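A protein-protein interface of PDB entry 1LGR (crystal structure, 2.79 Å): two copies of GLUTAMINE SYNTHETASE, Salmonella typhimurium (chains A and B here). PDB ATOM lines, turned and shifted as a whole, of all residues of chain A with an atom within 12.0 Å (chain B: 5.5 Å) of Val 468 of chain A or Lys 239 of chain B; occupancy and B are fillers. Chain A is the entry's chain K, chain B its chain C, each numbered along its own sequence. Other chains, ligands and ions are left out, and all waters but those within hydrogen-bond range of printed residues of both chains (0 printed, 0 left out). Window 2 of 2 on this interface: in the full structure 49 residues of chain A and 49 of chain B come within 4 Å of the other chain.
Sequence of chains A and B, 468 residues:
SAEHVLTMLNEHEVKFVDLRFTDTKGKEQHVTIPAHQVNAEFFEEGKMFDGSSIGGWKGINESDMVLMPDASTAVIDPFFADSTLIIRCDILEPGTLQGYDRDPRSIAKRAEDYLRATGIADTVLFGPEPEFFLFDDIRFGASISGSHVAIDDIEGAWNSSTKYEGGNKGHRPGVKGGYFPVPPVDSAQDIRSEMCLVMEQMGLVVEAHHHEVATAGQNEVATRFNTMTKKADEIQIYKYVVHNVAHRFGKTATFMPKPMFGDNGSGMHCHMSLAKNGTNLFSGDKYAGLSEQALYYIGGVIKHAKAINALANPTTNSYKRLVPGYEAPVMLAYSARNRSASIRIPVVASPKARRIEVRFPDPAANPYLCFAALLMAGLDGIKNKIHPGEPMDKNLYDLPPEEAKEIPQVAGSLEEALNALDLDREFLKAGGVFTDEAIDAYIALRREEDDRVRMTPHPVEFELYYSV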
ATOM      1  N   VAL A 460      11.238 -28.465 -11.478  1.00  0.00           N
ATOM      2  CA  VAL A 460      11.580 -27.046 -11.258  1.00  0.00           C
ATOM      3  C   VAL A 460      12.048 -26.293 -12.523  1.00  0.00           C
ATOM      4  O   VAL A 460      12.017 -25.064 -12.564  1.00  0.00           O
ATOM      5  CB  VAL A 460      12.666 -26.843 -10.139  1.00  0.00           C
ATOM      6  CG1 VAL A 460      12.292 -27.732  -8.973  1.00  0.00           C
ATOM      7  CG2 VAL A 460      14.056 -27.143 -10.593  1.00  0.00           C
ATOM      8  N   GLU A 461      12.404 -26.975 -13.627  1.00  0.00           N
ATOM      9  CA  GLU A 461      12.707 -26.274 -14.877  1.00  0.00           C
ATOM     10  C   GLU A 461      11.421 -25.611 -15.386  1.00  0.00           C
ATOM     11  O   GLU A 461      11.485 -24.479 -15.860  1.00  0.00           O
ATOM     12  CB  GLU A 461      13.221 -27.215 -15.965  1.00  0.00           C
ATOM     13  CG  GLU A 461      14.541 -27.823 -15.558  1.00  0.00           C
ATOM     14  CD  GLU A 461      15.225 -28.721 -16.584  1.00  0.00           C
ATOM     15  OE1 GLU A 461      14.559 -29.412 -17.357  1.00  0.00           O
ATOM     16  OE2 GLU A 461      16.452 -28.735 -16.601  1.00  0.00           O
ATOM     17  N   PHE A 462      10.225 -26.202 -15.248  1.00  0.00           N
ATOM     18  CA  PHE A 462       9.009 -25.499 -15.639  1.00  0.00           C
ATOM     19  C   PHE A 462       8.776 -24.285 -14.753  1.00  0.00           C
ATOM     20  O   PHE A 462       8.421 -23.200 -15.215  1.00  0.00           O
ATOM     21  CB  PHE A 462       7.829 -26.417 -15.545  1.00  0.00           C
ATOM     22  CG  PHE A 462       7.888 -27.354 -16.723  1.00  0.00           C
ATOM     23  CD1 PHE A 462       8.678 -28.495 -16.661  1.00  0.00           C
ATOM     24  CD2 PHE A 462       7.187 -27.040 -17.887  1.00  0.00           C
ATOM     25  CE1 PHE A 462       8.780 -29.330 -17.756  1.00  0.00           C
ATOM     26  CE2 PHE A 462       7.294 -27.880 -18.996  1.00  0.00           C
ATOM     27  CZ  PHE A 462       8.093 -29.023 -18.919  1.00  0.00           C
ATOM     28  N   GLU A 463       9.129 -24.426 -13.473  1.00  0.00           N
ATOM     29  CA  GLU A 463       9.041 -23.318 -12.521  1.00  0.00           C
ATOM     30  C   GLU A 463       9.932 -22.127 -12.899  1.00  0.00           C
ATOM     31  O   GLU A 463       9.558 -20.958 -12.852  1.00  0.00           O
ATOM     32  CB  GLU A 463       9.437 -23.849 -11.186  1.00  0.00           C
ATOM     33  CG  GLU A 463       8.829 -23.046 -10.096  1.00  0.00           C
ATOM     34  CD  GLU A 463       9.312 -23.584  -8.754  1.00  0.00           C
ATOM     35  OE1 GLU A 463       8.709 -24.545  -8.248  1.00  0.00           O
ATOM     36  OE2 GLU A 463      10.304 -23.045  -8.245  1.00  0.00           O
ATOM     37  N   LEU A 464      11.123 -22.491 -13.349  1.00  0.00           N
ATOM     38  CA  LEU A 464      12.170 -21.572 -13.764  1.00  0.00           C
ATOM     39  C   LEU A 464      12.055 -20.960 -15.155  1.00  0.00           C
ATOM     40  O   LEU A 464      12.255 -19.777 -15.411  1.00  0.00           O
ATOM     41  CB  LEU A 464      13.488 -22.324 -13.647  1.00  0.00           C
ATOM     42  CG  LEU A 464      14.464 -22.042 -12.512  1.00  0.00           C
ATOM     43  CD1 LEU A 464      13.758 -21.632 -11.245  1.00  0.00           C
ATOM     44  CD2 LEU A 464      15.275 -23.290 -12.287  1.00  0.00           C
ATOM     45  N   TYR A 465      11.688 -21.814 -16.097  1.00  0.00           N
ATOM     46  CA  TYR A 465      11.732 -21.468 -17.509  1.00  0.00           C
ATOM     47  C   TYR A 465      10.446 -21.531 -18.318  1.00  0.00           C
ATOM     48  O   TYR A 465      10.499 -21.248 -19.511  1.00  0.00           O
ATOM     49  CB  TYR A 465      12.763 -22.356 -18.202  1.00  0.00           C
ATOM     50  CG  TYR A 465      14.100 -22.382 -17.508  1.00  0.00           C
ATOM     51  CD1 TYR A 465      14.784 -21.204 -17.257  1.00  0.00           C
ATOM     52  CD2 TYR A 465      14.634 -23.600 -17.132  1.00  0.00           C
ATOM     53  CE1 TYR A 465      16.020 -21.240 -16.633  1.00  0.00           C
ATOM     54  CE2 TYR A 465      15.869 -23.646 -16.507  1.00  0.00           C
ATOM     55  CZ  TYR A 465      16.566 -22.466 -16.268  1.00  0.00           C
ATOM     56  OH  TYR A 465      17.849 -22.538 -15.757  1.00  0.00           O
ATOM     57  N   TYR A 466       9.261 -21.868 -17.796  1.00  0.00           N
ATOM     58  CA  TYR A 466       8.086 -21.909 -18.659  1.00  0.00           C
ATOM     59  C   TYR A 466       7.733 -20.542 -19.254  1.00  0.00           C
ATOM     60  O   TYR A 466       7.396 -20.398 -20.431  1.00  0.00           O
ATOM     61  CB  TYR A 466       6.891 -22.424 -17.878  1.00  0.00           C
ATOM     62  CG  TYR A 466       5.683 -22.661 -18.765  1.00  0.00           C
ATOM     63  CD1 TYR A 466       5.631 -23.780 -19.585  1.00  0.00           C
ATOM     64  CD2 TYR A 466       4.641 -21.735 -18.768  1.00  0.00           C
ATOM     65  CE1 TYR A 466       4.554 -23.981 -20.430  1.00  0.00           C
ATOM     66  CE2 TYR A 466       3.548 -21.919 -19.614  1.00  0.00           C
ATOM     67  CZ  TYR A 466       3.521 -23.049 -20.435  1.00  0.00           C
ATOM     68  OH  TYR A 466       2.448 -23.208 -21.286  1.00  0.00           O
ATOM     69  N   SER A 467       7.797 -19.491 -18.440  1.00  0.00           N
ATOM     70  CA  SER A 467       7.489 -18.170 -18.968  1.00  0.00           C
ATOM     71  C   SER A 467       8.629 -17.427 -19.637  1.00  0.00           C
ATOM     72  O   SER A 467       8.631 -16.194 -19.678  1.00  0.00           O
ATOM     73  CB  SER A 467       6.926 -17.293 -17.873  1.00  0.00           C
ATOM     74  OG  SER A 467       5.584 -17.699 -17.631  1.00  0.00           O
ATOM     75  N   VAL A 468       9.576 -18.220 -20.149  1.00  0.00           N
ATOM     76  CA  VAL A 468      10.655 -17.663 -20.941  1.00  0.00           C
ATOM     77  C   VAL A 468      10.047 -17.208 -22.306  1.00  0.00           C
ATOM     78  O   VAL A 468      10.589 -16.251 -22.864  1.00  0.00           O
ATOM     79  CB  VAL A 468      11.747 -18.781 -21.048  1.00  0.00           C
ATOM     80  CG1 VAL A 468      11.837 -19.497 -22.381  1.00  0.00           C
ATOM     81  CG2 VAL A 468      13.018 -18.082 -20.707  1.00  0.00           C
ATOM     82  OXT VAL A 468       8.998 -17.743 -22.761  1.00  0.00           O
ATOM     83  N   GLY B  26      16.413 -11.807 -20.071  1.00  0.00           N
ATOM     84  CA  GLY B  26      15.725 -11.739 -21.365  1.00  0.00           C
ATOM     85  C   GLY B  26      14.221 -11.421 -21.342  1.00  0.00           C
ATOM     86  O   GLY B  26      13.570 -11.266 -22.377  1.00  0.00           O
ATOM     87  N   LYS B  27      13.629 -11.322 -20.154  1.00  0.00           N
ATOM     88  CA  LYS B  27      12.229 -10.965 -20.019  1.00  0.00           C
ATOM     89  C   LYS B  27      11.955  -9.473 -20.152  1.00  0.00           C
ATOM     90  O   LYS B  27      12.564  -8.608 -19.503  1.00  0.00           O
ATOM     91  CB  LYS B  27      11.682 -11.434 -18.669  1.00  0.00           C
ATOM     92  CG  LYS B  27      10.148 -11.512 -18.580  1.00  0.00           C
ATOM     93  CD  LYS B  27       9.575 -12.524 -19.588  1.00  0.00           C
ATOM     94  CE  LYS B  27       8.047 -12.650 -19.554  1.00  0.00           C
ATOM     95  NZ  LYS B  27       7.548 -13.538 -20.599  1.00  0.00           N
ATOM     96  N   GLU B 234      12.778  -7.275 -32.374  1.00  0.00           N
ATOM     97  CA  GLU B 234      11.725  -8.029 -33.055  1.00  0.00           C
ATOM     98  C   GLU B 234      11.490  -9.402 -32.428  1.00  0.00           C
ATOM     99  O   GLU B 234      10.365  -9.895 -32.436  1.00  0.00           O
ATOM    100  CB  GLU B 234      12.054  -8.227 -34.521  1.00  0.00           C
ATOM    101  CG  GLU B 234      12.003  -6.911 -35.255  1.00  0.00           C
ATOM    102  CD  GLU B 234      12.137  -6.969 -36.778  1.00  0.00           C
ATOM    103  OE1 GLU B 234      12.231  -8.050 -37.355  1.00  0.00           O
ATOM    104  OE2 GLU B 234      12.125  -5.908 -37.401  1.00  0.00           O
ATOM    105  N   ILE B 235      12.509 -10.022 -31.824  1.00  0.00           N
ATOM    106  CA  ILE B 235      12.292 -11.247 -31.062  1.00  0.00           C
ATOM    107  C   ILE B 235      11.490 -10.921 -29.810  1.00  0.00           C
ATOM    108  O   ILE B 235      10.539 -11.640 -29.501  1.00  0.00           O
ATOM    109  CB  ILE B 235      13.642 -11.924 -30.681  1.00  0.00           C
ATOM    110  CG1 ILE B 235      14.228 -12.548 -31.932  1.00  0.00           C
ATOM    111  CG2 ILE B 235      13.470 -12.988 -29.616  1.00  0.00           C
ATOM    112  CD1 ILE B 235      13.227 -13.381 -32.747  1.00  0.00           C
ATOM    113  N   GLN B 236      11.774  -9.831 -29.091  1.00  0.00           N
ATOM    114  CA  GLN B 236      10.916  -9.454 -27.963  1.00  0.00           C
ATOM    115  C   GLN B 236       9.484  -9.160 -28.385  1.00  0.00           C
ATOM    116  O   GLN B 236       8.554  -9.524 -27.669  1.00  0.00           O
ATOM    117  CB  GLN B 236      11.469  -8.241 -27.265  1.00  0.00           C
ATOM    118  CG  GLN B 236      12.873  -8.523 -26.795  1.00  0.00           C
ATOM    119  CD  GLN B 236      12.922  -9.534 -25.668  1.00  0.00           C
ATOM    120  OE1 GLN B 236      12.958  -9.151 -24.516  1.00  0.00           O
ATOM    121  NE2 GLN B 236      12.906 -10.841 -25.797  1.00  0.00           N
ATOM    122  N   ILE B 237       9.228  -8.574 -29.560  1.00  0.00           N
ATOM    123  CA  ILE B 237       7.838  -8.452 -30.017  1.00  0.00           C
ATOM    124  C   ILE B 237       7.246  -9.796 -30.439  1.00  0.00           C
ATOM    125  O   ILE B 237       6.119 -10.134 -30.072  1.00  0.00           O
ATOM    126  CB  ILE B 237       7.774  -7.447 -31.177  1.00  0.00           C
ATOM    127  CG1 ILE B 237       8.021  -6.080 -30.552  1.00  0.00           C
ATOM    128  CG2 ILE B 237       6.442  -7.436 -31.908  1.00  0.00           C
ATOM    129  CD1 ILE B 237       8.348  -5.048 -31.612  1.00  0.00           C
ATOM    130  N   TYR B 238       8.028 -10.609 -31.146  1.00  0.00           N
ATOM    131  CA  TYR B 238       7.637 -11.948 -31.586  1.00  0.00           C
ATOM    132  C   TYR B 238       7.088 -12.776 -30.429  1.00  0.00           C
ATOM    133  O   TYR B 238       5.957 -13.269 -30.443  1.00  0.00           O
ATOM    134  CB  TYR B 238       8.838 -12.654 -32.159  1.00  0.00           C
ATOM    135  CG  TYR B 238       8.570 -14.030 -32.704  1.00  0.00           C
ATOM    136  CD1 TYR B 238       8.605 -15.157 -31.882  1.00  0.00           C
ATOM    137  CD2 TYR B 238       8.310 -14.153 -34.058  1.00  0.00           C
ATOM    138  CE1 TYR B 238       8.394 -16.423 -32.421  1.00  0.00           C
ATOM    139  CE2 TYR B 238       8.096 -15.418 -34.612  1.00  0.00           C
ATOM    140  CZ  TYR B 238       8.146 -16.542 -33.786  1.00  0.00           C
ATOM    141  OH  TYR B 238       7.994 -17.789 -34.340  1.00  0.00           O
ATOM    142  N   LYS B 239       7.919 -12.896 -29.396  1.00  0.00           N
ATOM    143  CA  LYS B 239       7.500 -13.574 -28.190  1.00  0.00           C
ATOM    144  C   LYS B 239       6.258 -12.948 -27.546  1.00  0.00           C
ATOM    145  O   LYS B 239       5.373 -13.695 -27.111  1.00  0.00           O
ATOM    146  CB  LYS B 239       8.587 -13.570 -27.146  1.00  0.00           C
ATOM    147  CG  LYS B 239       9.804 -14.458 -27.334  1.00  0.00           C
ATOM    148  CD  LYS B 239      10.410 -14.395 -25.948  1.00  0.00           C
ATOM    149  CE  LYS B 239      11.875 -14.766 -25.889  1.00  0.00           C
ATOM    150  NZ  LYS B 239      12.063 -16.084 -26.444  1.00  0.00           N
ATOM    151  N   TYR B 240       6.099 -11.617 -27.489  1.00  0.00           N
ATOM    152  CA  TYR B 240       4.919 -10.991 -26.877  1.00  0.00           C
ATOM    153  C   TYR B 240       3.620 -11.324 -27.602  1.00  0.00           C
ATOM    154  O   TYR B 240       2.599 -11.688 -27.022  1.00  0.00           O
ATOM    155  CB  TYR B 240       5.122  -9.477 -26.850  1.00  0.00           C
ATOM    156  CG  TYR B 240       3.998  -8.637 -26.263  1.00  0.00           C
ATOM    157  CD1 TYR B 240       3.705  -8.693 -24.904  1.00  0.00           C
ATOM    158  CD2 TYR B 240       3.275  -7.785 -27.090  1.00  0.00           C
ATOM    159  CE1 TYR B 240       2.704  -7.893 -24.370  1.00  0.00           C
ATOM    160  CE2 TYR B 240       2.268  -6.982 -26.566  1.00  0.00           C
ATOM    161  CZ  TYR B 240       2.000  -7.047 -25.207  1.00  0.00           C
ATOM    162  OH  TYR B 240       0.996  -6.280 -24.679  1.00  0.00           O
ATOM    163  N   VAL B 241       3.682 -11.264 -28.926  1.00  0.00           N
ATOM    164  CA  VAL B 241       2.527 -11.603 -29.738  1.00  0.00           C
ATOM    165  C   VAL B 241       2.196 -13.077 -29.588  1.00  0.00           C
ATOM    166  O   VAL B 241       1.038 -13.403 -29.335  1.00  0.00           O
ATOM    167  CB  VAL B 241       2.839 -11.241 -31.183  1.00  0.00           C
ATOM    168  CG1 VAL B 241       1.811 -11.756 -32.179  1.00  0.00           C
ATOM    169  CG2 VAL B 241       2.851  -9.725 -31.221  1.00  0.00           C
ATOM    170  N   VAL B 242       3.177 -13.984 -29.642  1.00  0.00           N
ATOM    171  CA  VAL B 242       2.887 -15.403 -29.450  1.00  0.00           C
ATOM    172  C   VAL B 242       2.251 -15.659 -28.089  1.00  0.00           C
ATOM    173  O   VAL B 242       1.152 -16.210 -28.007  1.00  0.00           O
ATOM    174  CB  VAL B 242       4.185 -16.199 -29.621  1.00  0.00           C
ATOM    175  CG1 VAL B 242       4.027 -17.654 -29.224  1.00  0.00           C
ATOM    176  CG2 VAL B 242       4.506 -16.230 -31.096  1.00  0.00           C
ATOM    177  N   HIS B 243       2.860 -15.154 -27.013  1.00  0.00           N
ATOM    178  CA  HIS B 243       2.290 -15.326 -25.676  1.00  0.00           C
ATOM    179  C   HIS B 243       0.870 -14.747 -25.582  1.00  0.00           C
ATOM    180  O   HIS B 243      -0.031 -15.438 -25.088  1.00  0.00           O
ATOM    181  CB  HIS B 243       3.150 -14.647 -24.608  1.00  0.00           C
ATOM    182  CG  HIS B 243       4.409 -15.415 -24.206  1.00  0.00           C
ATOM    183  ND1 HIS B 243       5.578 -14.894 -23.844  1.00  0.00           N
ATOM    184  CD2 HIS B 243       4.564 -16.780 -24.145  1.00  0.00           C
ATOM    185  CE1 HIS B 243       6.423 -15.860 -23.563  1.00  0.00           C
ATOM    186  NE2 HIS B 243       5.795 -16.986 -23.752  1.00  0.00           N
ATOM    187  N   ASN B 244       0.585 -13.553 -26.122  1.00  0.00           N
ATOM    188  CA  ASN B 244      -0.761 -13.012 -26.012  1.00  0.00           C
ATOM    189  C   ASN B 244      -1.829 -13.466 -26.994  1.00  0.00           C
ATOM    190  O   ASN B 244      -2.992 -13.576 -26.598  1.00  0.00           O
ATOM    191  CB  ASN B 244      -0.668 -11.527 -26.046  1.00  0.00           C
ATOM    192  CG  ASN B 244      -0.151 -11.072 -24.702  1.00  0.00           C
ATOM    193  OD1 ASN B 244       1.030 -11.037 -24.411  1.00  0.00           O
ATOM    194  ND2 ASN B 244      -0.993 -10.759 -23.749  1.00  0.00           N
ATOM    195  N   THR B 254       4.759 -21.459 -24.802  1.00  0.00           N
ATOM    196  CA  THR B 254       6.035 -21.442 -24.104  1.00  0.00           C
ATOM    197  C   THR B 254       7.255 -21.567 -25.008  1.00  0.00           C
ATOM    198  O   THR B 254       7.267 -22.327 -25.989  1.00  0.00           O
ATOM    199  CB  THR B 254       6.093 -22.569 -23.041  1.00  0.00           C
ATOM    200  OG1 THR B 254       7.329 -22.403 -22.376  1.00  0.00           O
ATOM    201  CG2 THR B 254       5.974 -23.972 -23.609  1.00  0.00           C
ATOM    202  N   PHE B 255       8.254 -20.748 -24.701  1.00  0.00           N
ATOM    203  CA  PHE B 255       9.491 -20.809 -25.443  1.00  0.00           C
ATOM    204  C   PHE B 255      10.559 -21.656 -24.762  1.00  0.00           C
ATOM    205  O   PHE B 255      11.743 -21.583 -25.135  1.00  0.00           O
ATOM    206  CB  PHE B 255      10.056 -19.417 -25.661  1.00  0.00           C
ATOM    207  CG  PHE B 255       9.200 -18.668 -26.653  1.00  0.00           C
ATOM    208  CD1 PHE B 255       9.334 -18.912 -28.026  1.00  0.00           C
ATOM    209  CD2 PHE B 255       8.241 -17.778 -26.167  1.00  0.00           C
ATOM    210  CE1 PHE B 255       8.486 -18.257 -28.914  1.00  0.00           C
ATOM    211  CE2 PHE B 255       7.406 -17.124 -27.075  1.00  0.00           C
ATOM    212  CZ  PHE B 255       7.525 -17.363 -28.445  1.00  0.00           C
ATOM    213  N   MET B 256      10.231 -22.495 -23.759  1.00  0.00           N
ATOM    214  CA  MET B 256      11.313 -23.253 -23.156  1.00  0.00           C
ATOM    215  C   MET B 256      11.792 -24.369 -24.090  1.00  0.00           C
ATOM    216  O   MET B 256      11.034 -24.927 -24.893  1.00  0.00           O
ATOM    217  CB  MET B 256      10.873 -23.807 -21.786  1.00  0.00           C
ATOM    218  CG  MET B 256      10.027 -25.048 -21.655  1.00  0.00           C
ATOM    219  SD  MET B 256       9.628 -25.359 -19.926  1.00  0.00           S
ATOM    220  CE  MET B 256      10.923 -26.456 -19.483  1.00  0.00           C
ATOM    221  N   PRO B 257      13.088 -24.675 -24.053  1.00  0.00           N
ATOM    222  CA  PRO B 257      13.783 -25.441 -25.091  1.00  0.00           C
ATOM    223  C   PRO B 257      13.284 -26.879 -25.228  1.00  0.00           C
ATOM    224  O   PRO B 257      13.034 -27.408 -26.306  1.00  0.00           O
ATOM    225  CB  PRO B 257      15.227 -25.379 -24.679  1.00  0.00           C
ATOM    226  CG  PRO B 257      15.310 -24.211 -23.723  1.00  0.00           C
ATOM    227  CD  PRO B 257      14.017 -24.293 -22.987  1.00  0.00           C
ATOM    228  N   MET B 268      16.126 -22.063 -31.538  1.00  0.00           N
ATOM    229  CA  MET B 268      16.081 -20.784 -32.244  1.00  0.00           C
ATOM    230  C   MET B 268      17.335 -20.647 -33.090  1.00  0.00           C
ATOM    231  O   MET B 268      18.371 -20.128 -32.677  1.00  0.00           O
ATOM    232  CB  MET B 268      16.021 -19.613 -31.274  1.00  0.00           C
ATOM    233  CG  MET B 268      15.857 -18.244 -31.915  1.00  0.00           C
ATOM    234  SD  MET B 268      16.512 -17.016 -30.768  1.00  0.00           S
ATOM    235  CE  MET B 268      15.011 -16.457 -30.039  1.00  0.00           C
ATOM    236  N   THR B 315      19.603 -21.926 -20.024  1.00  0.00           N
ATOM    237  CA  THR B 315      18.743 -22.560 -19.031  1.00  0.00           C
ATOM    238  C   THR B 315      19.193 -23.973 -18.736  1.00  0.00           C
ATOM    239  O   THR B 315      19.686 -24.613 -19.668  1.00  0.00           O
ATOM    240  CB  THR B 315      17.278 -22.653 -19.493  1.00  0.00           C
ATOM    241  OG1 THR B 315      17.181 -23.666 -20.467  1.00  0.00           O
ATOM    242  CG2 THR B 315      16.786 -21.357 -20.072  1.00  0.00           C
ATOM    243  N   PRO B 363      15.037 -20.549 -27.976  1.00  0.00           N
ATOM    244  CA  PRO B 363      14.195 -19.419 -27.594  1.00  0.00           C
ATOM    245  C   PRO B 363      14.373 -18.906 -26.176  1.00  0.00           C
ATOM    246  O   PRO B 363      14.019 -17.776 -25.891  1.00  0.00           O
ATOM    247  CB  PRO B 363      12.809 -19.898 -27.839  1.00  0.00           C
ATOM    248  CG  PRO B 363      12.969 -20.875 -28.957  1.00  0.00           C
ATOM    249  CD  PRO B 363      14.186 -21.617 -28.486  1.00  0.00           C
ATOM    250  N   ALA B 364      14.992 -19.663 -25.271  1.00  0.00           N
ATOM    251  CA  ALA B 364      15.210 -19.145 -23.930  1.00  0.00           C
ATOM    252  C   ALA B 364      16.299 -18.069 -23.826  1.00  0.00           C
ATOM    253  O   ALA B 364      16.460 -17.374 -22.820  1.00  0.00           O
ATOM    254  CB  ALA B 364      15.582 -20.284 -23.038  1.00  0.00           C
ATOM    255  N   ALA B 365      17.115 -17.971 -24.875  1.00  0.00           N
ATOM    256  CA  ALA B 365      18.215 -17.030 -24.913  1.00  0.00           C
ATOM    257  C   ALA B 365      17.822 -15.550 -24.947  1.00  0.00           C
ATOM    258  O   ALA B 365      16.852 -15.130 -25.590  1.00  0.00           O
ATOM    259  CB  ALA B 365      19.066 -17.329 -26.127  1.00  0.00           C
ATOM    260  N   PRO B 367      17.878 -12.341 -26.577  1.00  0.00           N
ATOM    261  CA  PRO B 367      18.236 -12.184 -27.978  1.00  0.00           C
ATOM    262  C   PRO B 367      19.343 -11.140 -28.135  1.00  0.00           C
ATOM    263  O   PRO B 367      20.261 -11.354 -28.923  1.00  0.00           O
ATOM    264  CB  PRO B 367      16.919 -11.844 -28.635  1.00  0.00           C
ATOM    265  CG  PRO B 367      16.152 -11.112 -27.561  1.00  0.00           C
ATOM    266  CD  PRO B 367      16.518 -11.886 -26.303  1.00  0.00           C
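Phe 462 of chain A touches Met 256 of chain B. Tyr 465 of chain A touches Met 256 of chain B (O to CB, 3.4 Å). Tyr 465 of chain A touches Thr 315 of chain B. Tyr 466 of chain A touches Met 256 of chain B (CA to SD, 3.99 Å). Val 468 of chain A touches Phe 255 of chain B. Val 468 of chain A touches Met 256 of chain B. Ala 364 of chain B touches Val 468 of chain A (CA to CG1, 3.7 Å).
O of Ser 467 of chain A is in hydrogen-bond range of NZ of Lys 27 of chain B, at 3.0 Å. The side-chain amino group (NZ) of Lys 239 of chain B is in salt-bridge range of the chain-end carboxylate (O) of Val 468 of chain A, at 3.9 Å. NE2 of His 243 of chain B sits close to OXT of Val 468 of chain A (3.4 Å). O of Tyr 466 of chain A sits at hydrogen-bond distance from OG1 of Thr 254 of chain B, 2.8 Å away.
Printed residues of chain B within 4 Å of Tyr 465 of chain A: Met 256 (3.4 Å) and Thr 315 (3.3 Å). Of the printed residues of chain B, Tyr 466 of chain A touches Thr 254 (2.8 Å) and Met 256 (3.99 Å). Printed residues of chain B within 4 Å of Ser 467 of chain A: Lys 27. No residue of chain A comes within 4 Å of Gly 26 of chain B. No residue of chain A comes within 4 Å of Ile 235 of chain B. No residue of chain A comes within 4 Å of Gln 236 of chain B. Tyr 238 of chain B touches none of the printed residues of chain A. Lys 239 of chain B touches one residue of chain A. No residue of chain A comes within 4 Å of Val 241 of chain B. No residue of chain A comes within 4 Å of Val 242 of chain B. His 243 of chain B touches one residue of chain A. Asn 244 of chain B touches none of the printed residues of chain A. Thr 254 of chain B touches one residue of chain A. No residue of chain A comes within 4 Å of Pro 363 of chain B. Of chain A, only Val 468 (3.7 Å) comes within 4 Å of Ala 364 of chain B. No residue of chain A comes within 4 Å of Ala 365 of chain B. The nearest residue of chain B that does not touch Val 468 of chain A is Pro 363 of chain B (4.5 Å). The nearest residue of chain A that does not touch Lys 239 of chain B is Ser 467 of chain A (6.8 Å).
No position is printed for both chains. Of the 11 pairs that touch across the chains among the printed residues, none has its exchanged pair printed and touching as well.
Hydrophobic or aromatic side chains of chain A that line the printed part of chain B: Phe 462, Tyr 465, Tyr 466 and Val 468. Printed residues of chain B that touch a printed residue of chain A: Lys 27, Lys 239, His 243, Thr 254, Phe 255, Met 256, Thr 315 and Ala 364. Along chain B the printed residues that touch a printed residue of chain A span positions 27 to 364. Among the printed residues, 11 pairs touch across the chains. Among the printed residues, no Asp or Glu carboxylate lies within 4 Å of a Lys or Arg side-chain nitrogen of the other chain.
The backbone carbonyl oxygen of Lys 239 of chain B sits close to a ring nitrogen (ND1) of His 243 of chain B, 3.5 Å away. NZ of Lys 239 of chain B lies within hydrogen-bond range of O of Pro 363 of chain B (2.6 Å). OG1 of Thr 254 of chain B sits at hydrogen-bond distance from N of Met 256 of chain B (3.2 Å).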
